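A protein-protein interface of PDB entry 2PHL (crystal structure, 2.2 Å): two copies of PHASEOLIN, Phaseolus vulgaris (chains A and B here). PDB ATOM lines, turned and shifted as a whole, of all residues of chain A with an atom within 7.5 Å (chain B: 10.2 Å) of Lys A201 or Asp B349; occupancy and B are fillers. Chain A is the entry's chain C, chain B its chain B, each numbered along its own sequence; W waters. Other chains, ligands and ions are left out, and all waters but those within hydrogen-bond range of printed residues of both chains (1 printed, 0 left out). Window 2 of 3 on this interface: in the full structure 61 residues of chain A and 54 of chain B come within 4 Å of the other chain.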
ATOM      1  N   TYR A  96       8.445  -1.734  -5.413  1.00  0.00           N
ATOM      2  CA  TYR A  96       7.561  -0.593  -5.170  1.00  0.00           C
ATOM      3  C   TYR A  96       6.137  -0.893  -5.526  1.00  0.00           C
ATOM      4  O   TYR A  96       5.893  -1.489  -6.561  1.00  0.00           O
ATOM      5  CB  TYR A  96       8.030   0.557  -6.030  1.00  0.00           C
ATOM      6  CG  TYR A  96       9.425   0.964  -5.718  1.00  0.00           C
ATOM      7  CD1 TYR A  96       9.681   1.877  -4.707  1.00  0.00           C
ATOM      8  CD2 TYR A  96      10.491   0.465  -6.451  1.00  0.00           C
ATOM      9  CE1 TYR A  96      10.959   2.287  -4.439  1.00  0.00           C
ATOM     10  CE2 TYR A  96      11.786   0.868  -6.193  1.00  0.00           C
ATOM     11  CZ  TYR A  96      12.014   1.784  -5.192  1.00  0.00           C
ATOM     12  OH  TYR A  96      13.283   2.267  -4.976  1.00  0.00           O
ATOM     13  N   TYR A 119       8.608  -0.466   4.357  1.00  0.00           N
ATOM     14  CA  TYR A 119       8.167   0.805   4.901  1.00  0.00           C
ATOM     15  C   TYR A 119       7.030   1.335   4.033  1.00  0.00           C
ATOM     16  O   TYR A 119       6.974   1.091   2.831  1.00  0.00           O
ATOM     17  CB  TYR A 119       9.315   1.807   5.134  1.00  0.00           C
ATOM     18  CG  TYR A 119      10.091   2.254   3.917  1.00  0.00           C
ATOM     19  CD1 TYR A 119       9.650   3.332   3.128  1.00  0.00           C
ATOM     20  CD2 TYR A 119      11.296   1.637   3.585  1.00  0.00           C
ATOM     21  CE1 TYR A 119      10.403   3.789   2.047  1.00  0.00           C
ATOM     22  CE2 TYR A 119      12.057   2.074   2.508  1.00  0.00           C
ATOM     23  CZ  TYR A 119      11.619   3.154   1.743  1.00  0.00           C
ATOM     24  OH  TYR A 119      12.446   3.616   0.729  1.00  0.00           O
ATOM     25  N   ASP A 196       7.684  15.339   3.980  1.00  0.00           N
ATOM     26  CA  ASP A 196       7.448  16.424   3.055  1.00  0.00           C
ATOM     27  C   ASP A 196       7.046  15.898   1.700  1.00  0.00           C
ATOM     28  O   ASP A 196       7.666  14.978   1.181  1.00  0.00           O
ATOM     29  CB  ASP A 196       8.736  17.204   2.884  1.00  0.00           C
ATOM     30  CG  ASP A 196       8.504  18.646   2.550  1.00  0.00           C
ATOM     31  OD1 ASP A 196       7.836  18.948   1.528  1.00  0.00           O
ATOM     32  OD2 ASP A 196       9.019  19.482   3.322  1.00  0.00           O
ATOM     33  N   SER A 197       6.059  16.549   1.097  1.00  0.00           N
ATOM     34  CA  SER A 197       5.570  16.195  -0.238  1.00  0.00           C
ATOM     35  C   SER A 197       6.724  16.200  -1.256  1.00  0.00           C
ATOM     36  O   SER A 197       6.784  15.380  -2.167  1.00  0.00           O
ATOM     37  CB  SER A 197       4.479  17.199  -0.671  1.00  0.00           C
ATOM     38  OG  SER A 197       4.685  18.494  -0.095  1.00  0.00           O
ATOM     39  N   GLU A 198       7.638  17.141  -1.070  1.00  0.00           N
ATOM     40  CA  GLU A 198       8.784  17.293  -1.936  1.00  0.00           C
ATOM     41  C   GLU A 198       9.746  16.132  -1.799  1.00  0.00           C
ATOM     42  O   GLU A 198      10.269  15.660  -2.794  1.00  0.00           O
ATOM     43  CB  GLU A 198       9.485  18.623  -1.651  1.00  0.00           C
ATOM     44  CG  GLU A 198       8.631  19.851  -1.992  1.00  0.00           C
ATOM     45  CD  GLU A 198       9.438  21.143  -2.066  1.00  0.00           C
ATOM     46  OE1 GLU A 198      10.338  21.251  -2.937  1.00  0.00           O
ATOM     47  OE2 GLU A 198       9.157  22.056  -1.259  1.00  0.00           O
ATOM     48  N   GLN A 199       9.970  15.659  -0.576  1.00  0.00           N
ATOM     49  CA  GLN A 199      10.880  14.532  -0.364  1.00  0.00           C
ATOM     50  C   GLN A 199      10.497  13.334  -1.254  1.00  0.00           C
ATOM     51  O   GLN A 199      11.289  12.877  -2.073  1.00  0.00           O
ATOM     52  CB  GLN A 199      10.888  14.091   1.115  1.00  0.00           C
ATOM     53  CG  GLN A 199      11.499  15.093   2.118  1.00  0.00           C
ATOM     54  CD  GLN A 199      11.508  14.594   3.577  1.00  0.00           C
ATOM     55  OE1 GLN A 199      10.491  14.640   4.277  1.00  0.00           O
ATOM     56  NE2 GLN A 199      12.669  14.147   4.040  1.00  0.00           N
ATOM     57  N   ILE A 200       9.254  12.876  -1.148  1.00  0.00           N
ATOM     58  CA  ILE A 200       8.809  11.725  -1.920  1.00  0.00           C
ATOM     59  C   ILE A 200       8.510  11.947  -3.404  1.00  0.00           C
ATOM     60  O   ILE A 200       7.830  11.120  -4.026  1.00  0.00           O
ATOM     61  CB  ILE A 200       7.601  11.056  -1.264  1.00  0.00           C
ATOM     62  CG1 ILE A 200       6.451  12.041  -1.131  1.00  0.00           C
ATOM     63  CG2 ILE A 200       7.976  10.552   0.098  1.00  0.00           C
ATOM     64  CD1 ILE A 200       5.142  11.368  -0.850  1.00  0.00           C
ATOM     65  N   LYS A 201       9.090  12.989  -3.994  1.00  0.00           N
ATOM     66  CA  LYS A 201       8.866  13.330  -5.407  1.00  0.00           C
ATOM     67  C   LYS A 201       9.216  12.215  -6.418  1.00  0.00           C
ATOM     68  O   LYS A 201       8.392  11.859  -7.267  1.00  0.00           O
ATOM     69  CB  LYS A 201       9.649  14.607  -5.754  1.00  0.00           C
ATOM     70  CG  LYS A 201       9.070  15.452  -6.887  1.00  0.00           C
ATOM     71  CD  LYS A 201       7.846  16.242  -6.437  1.00  0.00           C
ATOM     72  CE  LYS A 201       7.212  16.983  -7.606  1.00  0.00           C
ATOM     73  NZ  LYS A 201       6.680  16.058  -8.656  1.00  0.00           N
ATOM     74  N   GLU A 202      10.434  11.667  -6.310  1.00  0.00           N
ATOM     75  CA  GLU A 202      10.908  10.607  -7.211  1.00  0.00           C
ATOM     76  C   GLU A 202      10.110   9.320  -7.034  1.00  0.00           C
ATOM     77  O   GLU A 202       9.595   8.758  -7.998  1.00  0.00           O
ATOM     78  CB  GLU A 202      12.401  10.322  -6.971  1.00  0.00           C
ATOM     79  CG  GLU A 202      13.362  11.393  -7.505  1.00  0.00           C
ATOM     80  CD  GLU A 202      13.334  11.537  -9.034  1.00  0.00           C
ATOM     81  OE1 GLU A 202      13.331  10.503  -9.730  1.00  0.00           O
ATOM     82  OE2 GLU A 202      13.318  12.681  -9.550  1.00  0.00           O
ATOM     83  N   LEU A 203      10.004   8.902  -5.775  1.00  0.00           N
ATOM     84  CA  LEU A 203       9.308   7.695  -5.331  1.00  0.00           C
ATOM     85  C   LEU A 203       7.893   7.541  -5.917  1.00  0.00           C
ATOM     86  O   LEU A 203       7.623   6.634  -6.709  1.00  0.00           O
ATOM     87  CB  LEU A 203       9.206   7.742  -3.800  1.00  0.00           C
ATOM     88  CG  LEU A 203       9.207   6.535  -2.856  1.00  0.00           C
ATOM     89  CD1 LEU A 203       8.248   6.841  -1.710  1.00  0.00           C
ATOM     90  CD2 LEU A 203       8.819   5.249  -3.559  1.00  0.00           C
ATOM     91  N   SER A 204       6.987   8.407  -5.482  1.00  0.00           N
ATOM     92  CA  SER A 204       5.607   8.383  -5.921  1.00  0.00           C
ATOM     93  C   SER A 204       5.471   8.140  -7.416  1.00  0.00           C
ATOM     94  O   SER A 204       4.637   7.345  -7.850  1.00  0.00           O
ATOM     95  CB  SER A 204       4.967   9.707  -5.583  1.00  0.00           C
ATOM     96  OG  SER A 204       5.788  10.741  -6.084  1.00  0.00           O
ATOM     97  N   LYS A 205       6.290   8.827  -8.200  1.00  0.00           N
ATOM     98  CA  LYS A 205       6.246   8.686  -9.643  1.00  0.00           C
ATOM     99  C   LYS A 205       6.452   7.251 -10.064  1.00  0.00           C
ATOM    100  O   LYS A 205       5.598   6.673 -10.724  1.00  0.00           O
ATOM    101  CB  LYS A 205       7.301   9.568 -10.298  1.00  0.00           C
ATOM    102  CG  LYS A 205       7.106  11.053 -10.067  1.00  0.00           C
ATOM    103  CD  LYS A 205       8.302  11.839 -10.574  1.00  0.00           C
ATOM    104  CE  LYS A 205       8.592  11.535 -12.034  1.00  0.00           C
ATOM    105  NZ  LYS A 205       9.869  12.174 -12.418  1.00  0.00           N
ATOM    106  N   HIS A 206       7.567   6.658  -9.653  1.00  0.00           N
ATOM    107  CA  HIS A 206       7.859   5.278 -10.024  1.00  0.00           C
ATOM    108  C   HIS A 206       6.858   4.298  -9.449  1.00  0.00           C
ATOM    109  O   HIS A 206       6.592   3.241 -10.037  1.00  0.00           O
ATOM    110  CB  HIS A 206       9.250   4.861  -9.592  1.00  0.00           C
ATOM    111  CG  HIS A 206       9.581   3.455  -9.976  1.00  0.00           C
ATOM    112  ND1 HIS A 206       9.561   2.411  -9.075  1.00  0.00           N
ATOM    113  CD2 HIS A 206       9.867   2.907 -11.182  1.00  0.00           C
ATOM    114  CE1 HIS A 206       9.817   1.282  -9.710  1.00  0.00           C
ATOM    115  NE2 HIS A 206      10.007   1.557 -10.989  1.00  0.00           N
ATOM    116  N   LYS A 208       3.592   4.879  -8.880  1.00  0.00           N
ATOM    117  CA  LYS A 208       2.470   4.941  -9.802  1.00  0.00           C
ATOM    118  C   LYS A 208       2.748   4.406 -11.205  1.00  0.00           C
ATOM    119  O   LYS A 208       1.816   4.129 -11.944  1.00  0.00           O
ATOM    120  CB  LYS A 208       1.905   6.357  -9.880  1.00  0.00           C
ATOM    121  CG  LYS A 208       0.744   6.606  -8.916  1.00  0.00           C
ATOM    122  CD  LYS A 208       1.156   7.368  -7.659  1.00  0.00           C
ATOM    123  CE  LYS A 208       1.422   8.848  -7.945  1.00  0.00           C
ATOM    124  NZ  LYS A 208       1.623   9.629  -6.689  1.00  0.00           N
ATOM    125  N   SER B 342      22.209  -0.815   3.605  1.00  0.00           N
ATOM    126  CA  SER B 342      22.741  -0.147   2.411  1.00  0.00           C
ATOM    127  C   SER B 342      21.624  -0.183   1.380  1.00  0.00           C
ATOM    128  O   SER B 342      21.329   0.823   0.718  1.00  0.00           O
ATOM    129  CB  SER B 342      23.941  -0.889   1.836  1.00  0.00           C
ATOM    130  OG  SER B 342      25.051  -0.816   2.711  1.00  0.00           O
ATOM    131  N   SER B 343      20.979  -1.349   1.287  1.00  0.00           N
ATOM    132  CA  SER B 343      19.880  -1.543   0.358  1.00  0.00           C
ATOM    133  C   SER B 343      18.790  -0.512   0.586  1.00  0.00           C
ATOM    134  O   SER B 343      18.290   0.052  -0.381  1.00  0.00           O
ATOM    135  CB  SER B 343      19.318  -2.946   0.452  1.00  0.00           C
ATOM    136  OG  SER B 343      18.495  -3.194  -0.670  1.00  0.00           O
ATOM    137  N   ILE B 344      18.432  -0.247   1.849  1.00  0.00           N
ATOM    138  CA  ILE B 344      17.415   0.771   2.139  1.00  0.00           C
ATOM    139  C   ILE B 344      17.956   2.095   1.595  1.00  0.00           C
ATOM    140  O   ILE B 344      17.276   2.785   0.834  1.00  0.00           O
ATOM    141  CB  ILE B 344      17.106   0.974   3.677  1.00  0.00           C
ATOM    142  CG1 ILE B 344      16.410  -0.245   4.276  1.00  0.00           C
ATOM    143  CG2 ILE B 344      16.168   2.205   3.879  1.00  0.00           C
ATOM    144  CD1 ILE B 344      16.370  -0.224   5.788  1.00  0.00           C
ATOM    145  N   GLY B 345      19.191   2.416   1.966  1.00  0.00           N
ATOM    146  CA  GLY B 345      19.814   3.642   1.512  1.00  0.00           C
ATOM    147  C   GLY B 345      19.818   3.795   0.000  1.00  0.00           C
ATOM    148  O   GLY B 345      19.872   4.911  -0.499  1.00  0.00           O
ATOM    149  N   ARG B 346      19.733   2.692  -0.738  1.00  0.00           N
ATOM    150  CA  ARG B 346      19.747   2.760  -2.199  1.00  0.00           C
ATOM    151  C   ARG B 346      18.386   2.835  -2.910  1.00  0.00           C
ATOM    152  O   ARG B 346      18.318   2.987  -4.141  1.00  0.00           O
ATOM    153  CB  ARG B 346      20.647   1.655  -2.768  1.00  0.00           C
ATOM    154  CG  ARG B 346      22.149   1.962  -2.584  1.00  0.00           C
ATOM    155  CD  ARG B 346      23.015   0.747  -2.819  1.00  0.00           C
ATOM    156  NE  ARG B 346      22.881   0.201  -4.170  1.00  0.00           N
ATOM    157  CZ  ARG B 346      23.695   0.487  -5.192  1.00  0.00           C
ATOM    158  NH1 ARG B 346      24.714   1.325  -5.032  1.00  0.00           N
ATOM    159  NH2 ARG B 346      23.497  -0.072  -6.381  1.00  0.00           N
ATOM    160  N   ALA B 347      17.306   2.809  -2.129  1.00  0.00           N
ATOM    161  CA  ALA B 347      15.936   2.894  -2.662  1.00  0.00           C
ATOM    162  C   ALA B 347      15.746   4.260  -3.333  1.00  0.00           C
ATOM    163  O   ALA B 347      16.605   5.128  -3.192  1.00  0.00           O
ATOM    164  CB  ALA B 347      14.929   2.715  -1.512  1.00  0.00           C
ATOM    165  N   LEU B 348      14.600   4.500  -3.972  1.00  0.00           N
ATOM    166  CA  LEU B 348      14.373   5.797  -4.642  1.00  0.00           C
ATOM    167  C   LEU B 348      14.602   7.039  -3.787  1.00  0.00           C
ATOM    168  O   LEU B 348      15.512   7.834  -4.084  1.00  0.00           O
ATOM    169  CB  LEU B 348      13.038   5.863  -5.407  1.00  0.00           C
ATOM    170  CG  LEU B 348      13.152   5.166  -6.782  1.00  0.00           C
ATOM    171  CD1 LEU B 348      11.812   4.925  -7.395  1.00  0.00           C
ATOM    172  CD2 LEU B 348      14.066   5.940  -7.742  1.00  0.00           C
ATOM    173  N   ASP B 349      13.821   7.263  -2.742  1.00  0.00           N
ATOM    174  CA  ASP B 349      14.135   8.453  -1.931  1.00  0.00           C
ATOM    175  C   ASP B 349      14.796   7.999  -0.597  1.00  0.00           C
ATOM    176  O   ASP B 349      14.786   8.702   0.411  1.00  0.00           O
ATOM    177  CB  ASP B 349      12.884   9.363  -1.762  1.00  0.00           C
ATOM    178  CG  ASP B 349      12.619  10.288  -3.013  1.00  0.00           C
ATOM    179  OD1 ASP B 349      13.303  11.326  -3.143  1.00  0.00           O
ATOM    180  OD2 ASP B 349      11.726  10.014  -3.856  1.00  0.00           O
ATOM    181  N   GLY B 350      15.511   6.877  -0.689  1.00  0.00           N
ATOM    182  CA  GLY B 350      16.175   6.217   0.433  1.00  0.00           C
ATOM    183  C   GLY B 350      16.987   6.892   1.528  1.00  0.00           C
ATOM    184  O   GLY B 350      16.828   6.574   2.713  1.00  0.00           O
ATOM    185  N   LYS B 351      17.904   7.772   1.156  1.00  0.00           N
ATOM    186  CA  LYS B 351      18.733   8.447   2.157  1.00  0.00           C
ATOM    187  C   LYS B 351      17.858   9.224   3.142  1.00  0.00           C
ATOM    188  O   LYS B 351      18.186   9.314   4.331  1.00  0.00           O
ATOM    189  CB  LYS B 351      19.768   9.367   1.489  1.00  0.00           C
ATOM    190  CG  LYS B 351      20.689   8.647   0.505  1.00  0.00           C
ATOM    191  CD  LYS B 351      20.622   9.266  -0.913  1.00  0.00           C
ATOM    192  CE  LYS B 351      19.204   9.263  -1.559  1.00  0.00           C
ATOM    193  NZ  LYS B 351      18.684   7.906  -1.903  1.00  0.00           N
ATOM    194  N   ASP B 352      16.739   9.765   2.662  1.00  0.00           N
ATOM    195  CA  ASP B 352      15.833  10.486   3.540  1.00  0.00           C
ATOM    196  C   ASP B 352      15.215   9.520   4.572  1.00  0.00           C
ATOM    197  O   ASP B 352      14.956   9.902   5.719  1.00  0.00           O
ATOM    198  CB  ASP B 352      14.735  11.176   2.736  1.00  0.00           C
ATOM    199  CG  ASP B 352      15.249  12.360   1.933  1.00  0.00           C
ATOM    200  OD1 ASP B 352      15.901  13.260   2.521  1.00  0.00           O
ATOM    201  OD2 ASP B 352      14.980  12.392   0.713  1.00  0.00           O
ATOM    202  N   VAL B 353      14.981   8.276   4.167  1.00  0.00           N
ATOM    203  CA  VAL B 353      14.417   7.281   5.067  1.00  0.00           C
ATOM    204  C   VAL B 353      15.443   6.952   6.155  1.00  0.00           C
ATOM    205  O   VAL B 353      15.111   6.917   7.346  1.00  0.00           O
ATOM    206  CB  VAL B 353      14.009   6.011   4.293  1.00  0.00           C
ATOM    207  CG1 VAL B 353      13.636   4.886   5.237  1.00  0.00           C
ATOM    208  CG2 VAL B 353      12.842   6.324   3.405  1.00  0.00           C
ATOM    209  N   LEU B 354      16.699   6.755   5.755  1.00  0.00           N
ATOM    210  CA  LEU B 354      17.774   6.451   6.718  1.00  0.00           C
ATOM    211  C   LEU B 354      18.018   7.594   7.697  1.00  0.00           C
ATOM    212  O   LEU B 354      18.299   7.362   8.870  1.00  0.00           O
ATOM    213  CB  LEU B 354      19.090   6.138   6.002  1.00  0.00           C
ATOM    214  CG  LEU B 354      19.229   4.766   5.331  1.00  0.00           C
ATOM    215  CD1 LEU B 354      20.593   4.705   4.712  1.00  0.00           C
ATOM    216  CD2 LEU B 354      19.028   3.590   6.319  1.00  0.00           C
ATOM    217  N   GLY B 355      17.894   8.826   7.221  1.00  0.00           N
ATOM    218  CA  GLY B 355      18.118   9.957   8.083  1.00  0.00           C
ATOM    219  C   GLY B 355      17.041  10.111   9.133  1.00  0.00           C
ATOM    220  O   GLY B 355      17.275  10.743  10.165  1.00  0.00           O
ATOM    221  N   LEU B 356      15.856   9.570   8.851  1.00  0.00           N
ATOM    222  CA  LEU B 356      14.717   9.635   9.769  1.00  0.00           C
ATOM    223  C   LEU B 356      14.706   8.401  10.673  1.00  0.00           C
ATOM    224  O   LEU B 356      14.137   8.425  11.763  1.00  0.00           O
ATOM    225  CB  LEU B 356      13.398   9.721   8.987  1.00  0.00           C
ATOM    226  CG  LEU B 356      12.977  11.074   8.390  1.00  0.00           C
ATOM    227  CD1 LEU B 356      12.012  10.889   7.257  1.00  0.00           C
ATOM    228  CD2 LEU B 356      12.359  11.936   9.446  1.00  0.00           C
ATOM    229  N   THR B 357      15.371   7.339  10.230  1.00  0.00           N
ATOM    230  CA  THR B 357      15.447   6.085  10.980  1.00  0.00           C
ATOM    231  C   THR B 357      16.466   6.155  12.118  1.00  0.00           C
ATOM    232  O   THR B 357      16.246   5.631  13.203  1.00  0.00           O
ATOM    233  CB  THR B 357      15.871   4.949  10.032  1.00  0.00           C
ATOM    234  OG1 THR B 357      14.889   4.790   9.007  1.00  0.00           O
ATOM    235  CG2 THR B 357      16.054   3.648  10.780  1.00  0.00           C
ATOM    236  N   GLY B 362      21.340  10.773   6.275  1.00  0.00           N
ATOM    237  CA  GLY B 362      21.431   9.644   5.363  1.00  0.00           C
ATOM    238  C   GLY B 362      22.859   9.465   4.876  1.00  0.00           C
ATOM    239  O   GLY B 362      23.341   8.346   4.705  1.00  0.00           O
ATOM    240  N   ASP B 363      23.543  10.590   4.698  1.00  0.00           N
ATOM    241  CA  ASP B 363      24.918  10.626   4.238  1.00  0.00           C
ATOM    242  C   ASP B 363      25.821  10.073   5.328  1.00  0.00           C
ATOM    243  O   ASP B 363      26.669   9.233   5.058  1.00  0.00           O
ATOM    244  CB  ASP B 363      25.313  12.062   3.890  1.00  0.00           C
ATOM    245  CG  ASP B 363      24.421  12.675   2.796  1.00  0.00           C
ATOM    246  OD1 ASP B 363      24.574  12.276   1.618  1.00  0.00           O
ATOM    247  OD2 ASP B 363      23.574  13.557   3.107  1.00  0.00           O
ATOM    248  N   MET B 366      25.394   6.231   5.687  1.00  0.00           N
ATOM    249  CA  MET B 366      25.991   5.498   4.580  1.00  0.00           C
ATOM    250  C   MET B 366      27.498   5.444   4.758  1.00  0.00           C
ATOM    251  O   MET B 366      28.120   4.400   4.566  1.00  0.00           O
ATOM    252  CB  MET B 366      25.615   6.142   3.250  1.00  0.00           C
ATOM    253  CG  MET B 366      24.116   6.042   2.903  1.00  0.00           C
ATOM    254  SD  MET B 366      23.595   4.416   2.251  1.00  0.00           S
ATOM    255  CE  MET B 366      23.403   3.437   3.737  1.00  0.00           C
HETATM  256  O   HOH W   1      11.830   6.141  -0.286  1.00  0.00           O
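Tyr A96 touches Ala B347 (OH to C, 3.6 Å). Ala B347 touches Tyr A119. CE1 of Tyr A119 touches CG2 of Val B353 (3.8 Å). Gln A199 touches Asp B352 (NE2 to OD1, 3.7 Å). Asp B349 touches Ile A200. Lys A201 touches Asp B349. His A206 touches Leu B348.
Printed residues of chain B within 4 Å of Tyr A96: Ala B347 (3.6 Å) and Leu B348 (2.8 Å). Printed residues of chain B within 4 Å of Tyr A119: Ala B347 (3.5 Å) and Val B353 (3.8 Å). Ile A200 touches just one residue of chain B: Asp B349 (3.8 Å). Lys A201 touches just one residue of chain B: Asp B349. Ser A204 touches none of the printed residues of chain B. Printed residues of chain A within 4 Å of Asp B349: Gln A199, Ile A200, Lys A201, Glu A202 and Leu A203. Gly B350 touches none of the printed residues of chain A. Leu B356 touches none of the printed residues of chain A. The nearest residue of chain B that does not touch Lys A201 is Leu B348 (7.5 Å). The nearest printed residue of chain B that does not touch Tyr A119 is Ile B344 (4.3 Å).
No position is printed for both chains. Of the 11 pairs that touch across the chains among the printed residues, none has its exchanged pair printed and touching as well.
Water W1 lies within hydrogen-bond range of the side-chain hydroxyl of Tyr A119 (2.8 Å) and the backbone NH of Asp B349 (3.4 Å).
Of the 14 printed residues of chain A, 8 touch a printed residue of chain B. Hydrophobic or aromatic side chains of chain A that line the printed part of chain B: Tyr A96, Tyr A119, Leu A203 and His A206. Of the 19 printed residues of chain B, 5 touch a printed residue of chain A. Hydrophobic or aromatic side chains of chain B that line the printed part of chain A: Ala B347, Leu B348 and Val B353. Among the printed residues, no Asp or Glu carboxylate lies within 4 Å of a Lys or Arg side-chain nitrogen of the other chain.
The backbone NH of Leu B348 is in hydrogen-bond range of the side-chain hydroxyl of Tyr A96. The side-chain carboxylate (OD2) of Asp B349 sits close to the backbone NH (N) of Glu A202 (3.2 Å). The side-chain carboxylate (OD2) of Asp B349 is in hydrogen-bond range of the backbone NH (N) of Leu A203 (2.8 Å). OD1 of Asp B349 sits close to O of Gln A199 (2.8 Å).
O of Val B353 is in hydrogen-bond range of OG1 of Thr B357. The backbone NH of Asp A196 sits at hydrogen-bond distance from the side-chain amide oxygen of Gln A199, at 2.9 Å. The backbone carbonyl oxygen (O) of Ile A200 sits at hydrogen-bond distance from the side-chain hydroxyl (OG) of Ser A204, 2.9 Å away. O of Lys A201 is in hydrogen-bond range of OG of Ser A204 (3.1 Å).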
